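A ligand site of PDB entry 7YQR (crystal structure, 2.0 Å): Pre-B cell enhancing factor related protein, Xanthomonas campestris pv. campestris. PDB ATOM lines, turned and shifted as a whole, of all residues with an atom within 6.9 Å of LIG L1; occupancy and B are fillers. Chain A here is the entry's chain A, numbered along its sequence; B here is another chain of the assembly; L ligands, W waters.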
ATOM      1  N   HIS A 189     -17.602  23.597  -3.524  1.00  0.00           N
ATOM      2  CA  HIS A 189     -16.225  23.126  -3.378  1.00  0.00           C
ATOM      3  C   HIS A 189     -15.859  23.036  -1.890  1.00  0.00           C
ATOM      4  O   HIS A 189     -16.043  24.013  -1.139  1.00  0.00           O
ATOM      5  CB  HIS A 189     -15.275  24.083  -4.102  1.00  0.00           C
ATOM      6  CG  HIS A 189     -13.947  23.487  -4.411  1.00  0.00           C
ATOM      7  ND1 HIS A 189     -13.662  22.895  -5.632  1.00  0.00           N
ATOM      8  CD2 HIS A 189     -12.818  23.382  -3.675  1.00  0.00           C
ATOM      9  CE1 HIS A 189     -12.422  22.455  -5.619  1.00  0.00           C
ATOM     10  NE2 HIS A 189     -11.883  22.739  -4.444  1.00  0.00           N
ATOM     11  N   ASP A 190     -15.338  21.891  -1.460  1.00  0.00           N
ATOM     12  CA  ASP A 190     -14.960  21.705  -0.051  1.00  0.00           C
ATOM     13  C   ASP A 190     -13.660  22.440   0.255  1.00  0.00           C
ATOM     14  O   ASP A 190     -12.620  22.105  -0.312  1.00  0.00           O
ATOM     15  CB  ASP A 190     -14.824  20.211   0.229  1.00  0.00           C
ATOM     16  CG  ASP A 190     -14.409  19.906   1.685  1.00  0.00           C
ATOM     17  OD1 ASP A 190     -14.449  20.795   2.553  1.00  0.00           O
ATOM     18  OD2 ASP A 190     -14.057  18.728   1.930  1.00  0.00           O
ATOM     19  N   PHE A 191     -13.723  23.427   1.161  1.00  0.00           N
ATOM     20  CA  PHE A 191     -12.566  24.145   1.698  1.00  0.00           C
ATOM     21  C   PHE A 191     -12.254  23.774   3.154  1.00  0.00           C
ATOM     22  O   PHE A 191     -11.514  24.505   3.816  1.00  0.00           O
ATOM     23  CB  PHE A 191     -12.783  25.670   1.669  1.00  0.00           C
ATOM     24  CG  PHE A 191     -12.641  26.333   0.309  1.00  0.00           C
ATOM     25  CD1 PHE A 191     -12.336  25.610  -0.823  1.00  0.00           C
ATOM     26  CD2 PHE A 191     -12.815  27.704   0.186  1.00  0.00           C
ATOM     27  CE1 PHE A 191     -12.217  26.234  -2.068  1.00  0.00           C
ATOM     28  CE2 PHE A 191     -12.696  28.343  -1.050  1.00  0.00           C
ATOM     29  CZ  PHE A 191     -12.395  27.612  -2.179  1.00  0.00           C
ATOM     30  N   GLY A 192     -12.827  22.701   3.677  1.00  0.00           N
ATOM     31  CA  GLY A 192     -12.870  22.539   5.112  1.00  0.00           C
ATOM     32  C   GLY A 192     -11.741  21.809   5.828  1.00  0.00           C
ATOM     33  O   GLY A 192     -11.841  21.652   7.044  1.00  0.00           O
ATOM     34  N   ALA A 193     -10.685  21.372   5.138  1.00  0.00           N
ATOM     35  CA  ALA A 193      -9.692  20.497   5.759  1.00  0.00           C
ATOM     36  C   ALA A 193      -9.008  21.161   6.975  1.00  0.00           C
ATOM     37  O   ALA A 193      -8.748  20.501   7.982  1.00  0.00           O
ATOM     38  CB  ALA A 193      -8.667  20.059   4.719  1.00  0.00           C
ATOM     39  N   ARG A 194      -8.739  22.467   6.901  1.00  0.00           N
ATOM     40  CA  ARG A 194      -8.138  23.178   8.035  1.00  0.00           C
ATOM     41  C   ARG A 194      -9.126  23.475   9.160  1.00  0.00           C
ATOM     42  O   ARG A 194      -8.697  23.770  10.282  1.00  0.00           O
ATOM     43  CB  ARG A 194      -7.499  24.492   7.578  1.00  0.00           C
ATOM     44  CG  ARG A 194      -8.510  25.628   7.396  1.00  0.00           C
ATOM     45  CD  ARG A 194      -7.959  26.809   6.601  1.00  0.00           C
ATOM     46  NE  ARG A 194      -7.339  26.390   5.348  1.00  0.00           N
ATOM     47  CZ  ARG A 194      -6.567  27.178   4.597  1.00  0.00           C
ATOM     48  NH1 ARG A 194      -6.335  28.418   4.980  1.00  0.00           N
ATOM     49  NH2 ARG A 194      -6.015  26.716   3.481  1.00  0.00           N
ATOM     50  N   ASP A 217     -10.886  20.570  -2.182  1.00  0.00           N
ATOM     51  CA  ASP A 217      -9.496  20.767  -1.796  1.00  0.00           C
ATOM     52  C   ASP A 217      -9.059  19.837  -0.668  1.00  0.00           C
ATOM     53  O   ASP A 217      -7.917  19.916  -0.210  1.00  0.00           O
ATOM     54  CB  ASP A 217      -9.251  22.231  -1.399  1.00  0.00           C
ATOM     55  CG  ASP A 217      -8.814  23.101  -2.569  1.00  0.00           C
ATOM     56  OD1 ASP A 217      -9.342  22.962  -3.695  1.00  0.00           O
ATOM     57  OD2 ASP A 217      -7.915  23.926  -2.345  1.00  0.00           O
ATOM     58  N   SER A 237      -9.584  19.588  -8.464  1.00  0.00           N
ATOM     59  CA  SER A 237      -9.440  20.973  -8.066  1.00  0.00           C
ATOM     60  C   SER A 237      -8.587  21.692  -9.107  1.00  0.00           C
ATOM     61  O   SER A 237      -8.263  21.132 -10.163  1.00  0.00           O
ATOM     62  CB  SER A 237      -8.852  21.089  -6.643  1.00  0.00           C
ATOM     63  OG  SER A 237      -8.908  22.441  -6.229  1.00  0.00           O
ATOM     64  N   ILE A 238      -8.232  22.934  -8.800  1.00  0.00           N
ATOM     65  CA  ILE A 238      -7.493  23.811  -9.706  1.00  0.00           C
ATOM     66  C   ILE A 238      -6.416  24.545  -8.927  1.00  0.00           C
ATOM     67  O   ILE A 238      -6.451  24.613  -7.687  1.00  0.00           O
ATOM     68  CB  ILE A 238      -8.420  24.840 -10.392  1.00  0.00           C
ATOM     69  CG1 ILE A 238      -9.097  25.721  -9.343  1.00  0.00           C
ATOM     70  CG2 ILE A 238      -9.453  24.150 -11.307  1.00  0.00           C
ATOM     71  CD1 ILE A 238      -9.938  26.845  -9.917  1.00  0.00           C
ATOM     72  N   PRO A 239      -5.413  25.106  -9.622  1.00  0.00           N
ATOM     73  CA  PRO A 239      -4.466  26.006  -8.956  1.00  0.00           C
ATOM     74  C   PRO A 239      -5.188  27.227  -8.439  1.00  0.00           C
ATOM     75  O   PRO A 239      -6.103  27.734  -9.080  1.00  0.00           O
ATOM     76  CB  PRO A 239      -3.453  26.371 -10.055  1.00  0.00           C
ATOM     77  CG  PRO A 239      -3.695  25.422 -11.175  1.00  0.00           C
ATOM     78  CD  PRO A 239      -5.108  24.908 -11.059  1.00  0.00           C
ATOM     79  N   ALA A 240      -4.781  27.710  -7.261  1.00  0.00           N
ATOM     80  CA  ALA A 240      -5.445  28.856  -6.646  1.00  0.00           C
ATOM     81  C   ALA A 240      -4.458  29.641  -5.792  1.00  0.00           C
ATOM     82  O   ALA A 240      -3.599  29.055  -5.125  1.00  0.00           O
ATOM     83  CB  ALA A 240      -6.640  28.431  -5.790  1.00  0.00           C
ATOM     84  N   ALA A 241      -4.611  30.965  -5.795  1.00  0.00           N
ATOM     85  CA  ALA A 241      -3.723  31.844  -5.045  1.00  0.00           C
ATOM     86  C   ALA A 241      -4.093  31.879  -3.565  1.00  0.00           C
ATOM     87  O   ALA A 241      -5.258  31.746  -3.177  1.00  0.00           O
ATOM     88  CB  ALA A 241      -3.778  33.269  -5.614  1.00  0.00           C
ATOM     89  N   GLU A 242      -3.069  32.049  -2.749  1.00  0.00           N
ATOM     90  CA  GLU A 242      -3.192  32.371  -1.335  1.00  0.00           C
ATOM     91  C   GLU A 242      -2.992  33.865  -1.166  1.00  0.00           C
ATOM     92  O   GLU A 242      -1.993  34.411  -1.658  1.00  0.00           O
ATOM     93  CB  GLU A 242      -2.155  31.589  -0.538  1.00  0.00           C
ATOM     94  CG  GLU A 242      -2.414  31.456   0.932  1.00  0.00           C
ATOM     95  CD  GLU A 242      -1.464  30.459   1.548  1.00  0.00           C
ATOM     96  OE1 GLU A 242      -1.728  29.250   1.450  1.00  0.00           O
ATOM     97  OE2 GLU A 242      -0.423  30.903   2.113  1.00  0.00           O
ATOM     98  N   ALA A 273      -7.786  30.106 -10.059  1.00  0.00           N
ATOM     99  CA  ALA A 273      -8.519  30.959  -9.126  1.00  0.00           C
ATOM    100  C   ALA A 273      -7.588  32.013  -8.511  1.00  0.00           C
ATOM    101  O   ALA A 273      -6.449  31.707  -8.133  1.00  0.00           O
ATOM    102  CB  ALA A 273      -9.166  30.123  -8.024  1.00  0.00           C
ATOM    103  N   VAL A 275      -7.529  35.207  -5.563  1.00  0.00           N
ATOM    104  CA  VAL A 275      -8.193  35.801  -4.408  1.00  0.00           C
ATOM    105  C   VAL A 275      -7.804  37.271  -4.362  1.00  0.00           C
ATOM    106  O   VAL A 275      -6.672  37.624  -4.716  1.00  0.00           O
ATOM    107  CB  VAL A 275      -7.837  35.055  -3.098  1.00  0.00           C
ATOM    108  CG1 VAL A 275      -6.334  35.088  -2.834  1.00  0.00           C
ATOM    109  CG2 VAL A 275      -8.616  35.626  -1.910  1.00  0.00           C
ATOM    110  N   ARG A 307     -12.067  35.244  -6.473  1.00  0.00           N
ATOM    111  CA  ARG A 307     -12.609  34.975  -5.145  1.00  0.00           C
ATOM    112  C   ARG A 307     -12.499  36.222  -4.290  1.00  0.00           C
ATOM    113  O   ARG A 307     -11.401  36.546  -3.807  1.00  0.00           O
ATOM    114  CB  ARG A 307     -11.875  33.809  -4.484  1.00  0.00           C
ATOM    115  CG  ARG A 307     -12.394  33.514  -3.072  1.00  0.00           C
ATOM    116  CD  ARG A 307     -11.887  32.176  -2.572  1.00  0.00           C
ATOM    117  NE  ARG A 307     -10.916  32.356  -1.492  1.00  0.00           N
ATOM    118  CZ  ARG A 307      -9.630  32.063  -1.622  1.00  0.00           C
ATOM    119  NH1 ARG A 307      -9.179  31.600  -2.782  1.00  0.00           N
ATOM    120  NH2 ARG A 307      -8.805  32.244  -0.611  1.00  0.00           N
ATOM    121  N   ILE A 346     -16.111  32.808  -7.257  1.00  0.00           N
ATOM    122  CA  ILE A 346     -16.385  31.870  -6.170  1.00  0.00           C
ATOM    123  C   ILE A 346     -16.410  32.648  -4.860  1.00  0.00           C
ATOM    124  O   ILE A 346     -15.527  33.470  -4.607  1.00  0.00           O
ATOM    125  CB  ILE A 346     -15.376  30.714  -6.106  1.00  0.00           C
ATOM    126  CG1 ILE A 346     -15.831  29.711  -5.028  1.00  0.00           C
ATOM    127  CG2 ILE A 346     -13.966  31.221  -5.812  1.00  0.00           C
ATOM    128  CD1 ILE A 346     -15.252  28.338  -5.171  1.00  0.00           C
ATOM    129  N   GLY A 348     -16.030  32.057  -1.048  1.00  0.00           N
ATOM    130  CA  GLY A 348     -15.604  31.128  -0.026  1.00  0.00           C
ATOM    131  C   GLY A 348     -15.756  31.618   1.385  1.00  0.00           C
ATOM    132  O   GLY A 348     -15.208  30.991   2.306  1.00  0.00           O
ATOM    133  N   ASP B  26      -4.320  21.095   1.866  1.00  0.00           N
ATOM    134  CA  ASP B  26      -5.300  21.556   0.896  1.00  0.00           C
ATOM    135  C   ASP B  26      -4.737  21.438  -0.512  1.00  0.00           C
ATOM    136  O   ASP B  26      -3.563  21.741  -0.755  1.00  0.00           O
ATOM    137  CB  ASP B  26      -5.670  23.027   1.142  1.00  0.00           C
ATOM    138  CG  ASP B  26      -6.413  23.230   2.439  1.00  0.00           C
ATOM    139  OD1 ASP B  26      -7.510  22.644   2.605  1.00  0.00           O
ATOM    140  OD2 ASP B  26      -5.905  23.999   3.295  1.00  0.00           O
ATOM    141  N   SER B  27      -5.600  21.028  -1.459  1.00  0.00           N
ATOM    142  CA  SER B  27      -5.161  20.818  -2.842  1.00  0.00           C
ATOM    143  C   SER B  27      -4.348  22.001  -3.377  1.00  0.00           C
ATOM    144  O   SER B  27      -3.292  21.816  -3.997  1.00  0.00           O
ATOM    145  CB  SER B  27      -6.384  20.596  -3.749  1.00  0.00           C
ATOM    146  OG  SER B  27      -7.056  19.402  -3.395  1.00  0.00           O
ATOM    147  N   TYR B  28      -4.829  23.220  -3.163  1.00  0.00           N
ATOM    148  CA  TYR B  28      -4.170  24.363  -3.790  1.00  0.00           C
ATOM    149  C   TYR B  28      -2.769  24.621  -3.231  1.00  0.00           C
ATOM    150  O   TYR B  28      -1.992  25.357  -3.866  1.00  0.00           O
ATOM    151  CB  TYR B  28      -5.045  25.616  -3.641  1.00  0.00           C
ATOM    152  CG  TYR B  28      -5.016  26.330  -2.302  1.00  0.00           C
ATOM    153  CD1 TYR B  28      -5.391  25.691  -1.130  1.00  0.00           C
ATOM    154  CD2 TYR B  28      -4.654  27.668  -2.234  1.00  0.00           C
ATOM    155  CE1 TYR B  28      -5.376  26.366   0.090  1.00  0.00           C
ATOM    156  CE2 TYR B  28      -4.623  28.333  -1.019  1.00  0.00           C
ATOM    157  CZ  TYR B  28      -4.986  27.682   0.138  1.00  0.00           C
ATOM    158  OH  TYR B  28      -4.971  28.371   1.334  1.00  0.00           O
ATOM    159  N   LYS B  29      -2.424  24.027  -2.095  1.00  0.00           N
ATOM    160  CA  LYS B  29      -1.070  24.161  -1.551  1.00  0.00           C
ATOM    161  C   LYS B  29      -0.045  23.465  -2.429  1.00  0.00           C
ATOM    162  O   LYS B  29       1.130  23.830  -2.417  1.00  0.00           O
ATOM    163  CB  LYS B  29      -1.007  23.595  -0.131  1.00  0.00           C
ATOM    164  CG  LYS B  29      -1.935  24.292   0.848  1.00  0.00           C
ATOM    165  CD  LYS B  29      -1.360  25.593   1.292  1.00  0.00           C
ATOM    166  CE  LYS B  29      -2.016  26.070   2.584  1.00  0.00           C
ATOM    167  NZ  LYS B  29      -1.444  27.391   2.982  1.00  0.00           N
ATOM    168  N   GLU B  91      -3.693  19.346  -9.901  1.00  0.00           N
ATOM    169  CA  GLU B  91      -2.751  20.313  -9.344  1.00  0.00           C
ATOM    170  C   GLU B  91      -1.339  20.077  -9.869  1.00  0.00           C
ATOM    171  O   GLU B  91      -0.931  18.928 -10.028  1.00  0.00           O
ATOM    172  CB  GLU B  91      -2.700  20.240  -7.799  1.00  0.00           C
ATOM    173  CG  GLU B  91      -4.005  20.536  -7.065  1.00  0.00           C
ATOM    174  CD  GLU B  91      -4.346  21.999  -7.052  1.00  0.00           C
ATOM    175  OE1 GLU B  91      -3.494  22.824  -7.447  1.00  0.00           O
ATOM    176  OE2 GLU B  91      -5.473  22.340  -6.646  1.00  0.00           O
ATOM    177  N   THR B 147      -2.449  23.553   6.731  1.00  0.00           N
ATOM    178  CA  THR B 147      -3.700  22.822   6.900  1.00  0.00           C
ATOM    179  C   THR B 147      -3.657  21.904   8.121  1.00  0.00           C
ATOM    180  O   THR B 147      -4.577  21.922   8.951  1.00  0.00           O
ATOM    181  CB  THR B 147      -3.970  22.000   5.639  1.00  0.00           C
ATOM    182  OG1 THR B 147      -3.767  22.827   4.479  1.00  0.00           O
ATOM    183  CG2 THR B 147      -5.383  21.445   5.651  1.00  0.00           C
ATOM    184  N   ARG B 387     -13.624  26.179  14.248  1.00  0.00           N
ATOM    185  CA  ARG B 387     -12.453  27.053  14.157  1.00  0.00           C
ATOM    186  C   ARG B 387     -12.811  28.513  14.421  1.00  0.00           C
ATOM    187  O   ARG B 387     -11.926  29.308  14.733  1.00  0.00           O
ATOM    188  CB  ARG B 387     -11.797  26.911  12.778  1.00  0.00           C
ATOM    189  CG  ARG B 387     -10.504  27.714  12.635  1.00  0.00           C
ATOM    190  CD  ARG B 387      -9.656  27.280  11.462  1.00  0.00           C
ATOM    191  NE  ARG B 387     -10.215  27.729  10.188  1.00  0.00           N
ATOM    192  CZ  ARG B 387      -9.884  28.855   9.575  1.00  0.00           C
ATOM    193  NH1 ARG B 387      -9.001  29.688  10.104  1.00  0.00           N
ATOM    194  NH2 ARG B 387     -10.455  29.151   8.410  1.00  0.00           N
HETATM  195  N1  LIG L   1      -9.348  28.060   1.679  1.00  0.00           N
HETATM  196  C1  LIG L   1      -9.175  28.292   0.352  1.00  0.00           C
HETATM  197  C2  LIG L   1      -8.930  27.240  -0.513  1.00  0.00           C
HETATM  198  C3  LIG L   1      -8.845  25.975  -0.016  1.00  0.00           C
HETATM  199  C4  LIG L   1      -9.027  25.748   1.314  1.00  0.00           C
HETATM  200  C5  LIG L   1      -9.272  26.808   2.166  1.00  0.00           C
HETATM  201  C6  LIG L   1      -8.725  27.474  -2.009  1.00  0.00           C
HETATM  202  O1  LIG L   1      -8.752  28.580  -2.473  1.00  0.00           O
HETATM  203  N2  LIG L   1      -8.470  26.322  -2.873  1.00  0.00           N
HETATM  204  N1  LG2 L   2     -11.566  25.704  -6.406  1.00  0.00           N
HETATM  205  C1  LG2 L   2     -12.656  25.699  -7.219  1.00  0.00           C
HETATM  206  C2  LG2 L   2     -13.204  26.896  -7.646  1.00  0.00           C
HETATM  207  C3  LG2 L   2     -12.607  28.063  -7.245  1.00  0.00           C
HETATM  208  C4  LG2 L   2     -11.525  28.058  -6.438  1.00  0.00           C
HETATM  209  C5  LG2 L   2     -10.981  26.874  -6.012  1.00  0.00           C
HETATM  210  C6  LG2 L   2     -14.442  26.942  -8.556  1.00  0.00           C
HETATM  211  O1  LG2 L   2     -14.785  27.982  -9.026  1.00  0.00           O
HETATM  212  N2  LG2 L   2     -15.234  25.747  -8.856  1.00  0.00           N
HETATM  213  O   HOH W   1      -8.141  25.091  -5.358  1.00  0.00           O
HETATM  214  O   HOH W   2      -7.241  30.436  -1.656  1.00  0.00           O
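N of Tyr 28 of chain B lies within hydrogen-bond range of OD2 of Asp 217 (3.3 Å). The side-chain carboxylate (OD1) of Asp 217 lies within hydrogen-bond range of the side-chain hydroxyl (OG) of Ser 237 (2.6 Å). A ring nitrogen (NE2) of His 189 lies within hydrogen-bond range of the side-chain carboxylate of Asp 217 (2.7 Å). O of Asp 190 sits at hydrogen-bond distance from N of Asp 217 (3.0 Å). The backbone carbonyl oxygen of Asp 217 sits at hydrogen-bond distance from the backbone NH of Ser 27 of chain B (2.9 Å). The guanidinium group (NH2) of Arg 194 is in hydrogen-bond range of the side-chain hydroxyl (OH) of Tyr 28 of chain B, at 2.9 Å. NH2 of Arg 194 lies within salt-bridge range of OD2 of Asp 26 of chain B, at 2.7 Å. OD2 of Asp 26 of chain B sits at hydrogen-bond distance from OG1 of Thr 147 of chain B, 2.7 Å away.
Water W2 lies within hydrogen-bond range of the guanidinium group of Arg 307 (2.5 Å), an oxygen (O1) of LIG L1 (2.5 Å) and the backbone carbonyl oxygen of Ala 241 (2.8 Å). Water W1 lies within hydrogen-bond range of N2 of LIG L1 (2.8 Å), OG of Ser 237 (2.9 Å), O of Ile 238 (2.9 Å) and OD1 of Asp 217 (3.0 Å).
A nitrogen (N2) of LIG L1 lies within hydrogen-bond range of the side-chain carboxylate (OD2) of Asp 217, 2.5 Å away. The guanidinium group (NH1) of Arg 307 sits at hydrogen-bond distance from an oxygen (O1) of LIG L1.
Residues that only touch LIG L1: Phe 191 (3.6 Å), Arg 194 (3.5 Å), Ala 240 (3.9 Å), Asp 26 of chain B (3.7 Å) and Tyr 28 of chain B (3.5 Å). Seven residues have an atom within 4 Å of LIG L1: Phe 191, Arg 194, Asp 217, Ala 240, Arg 307, Asp 26 of chain B and Tyr 28 of chain B. Along chain A the residues within 4 Å of LIG L1 span positions 191 to 307. The nearest printed residue that does not touch LIG L1 is Ala 241 (4.8 Å).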
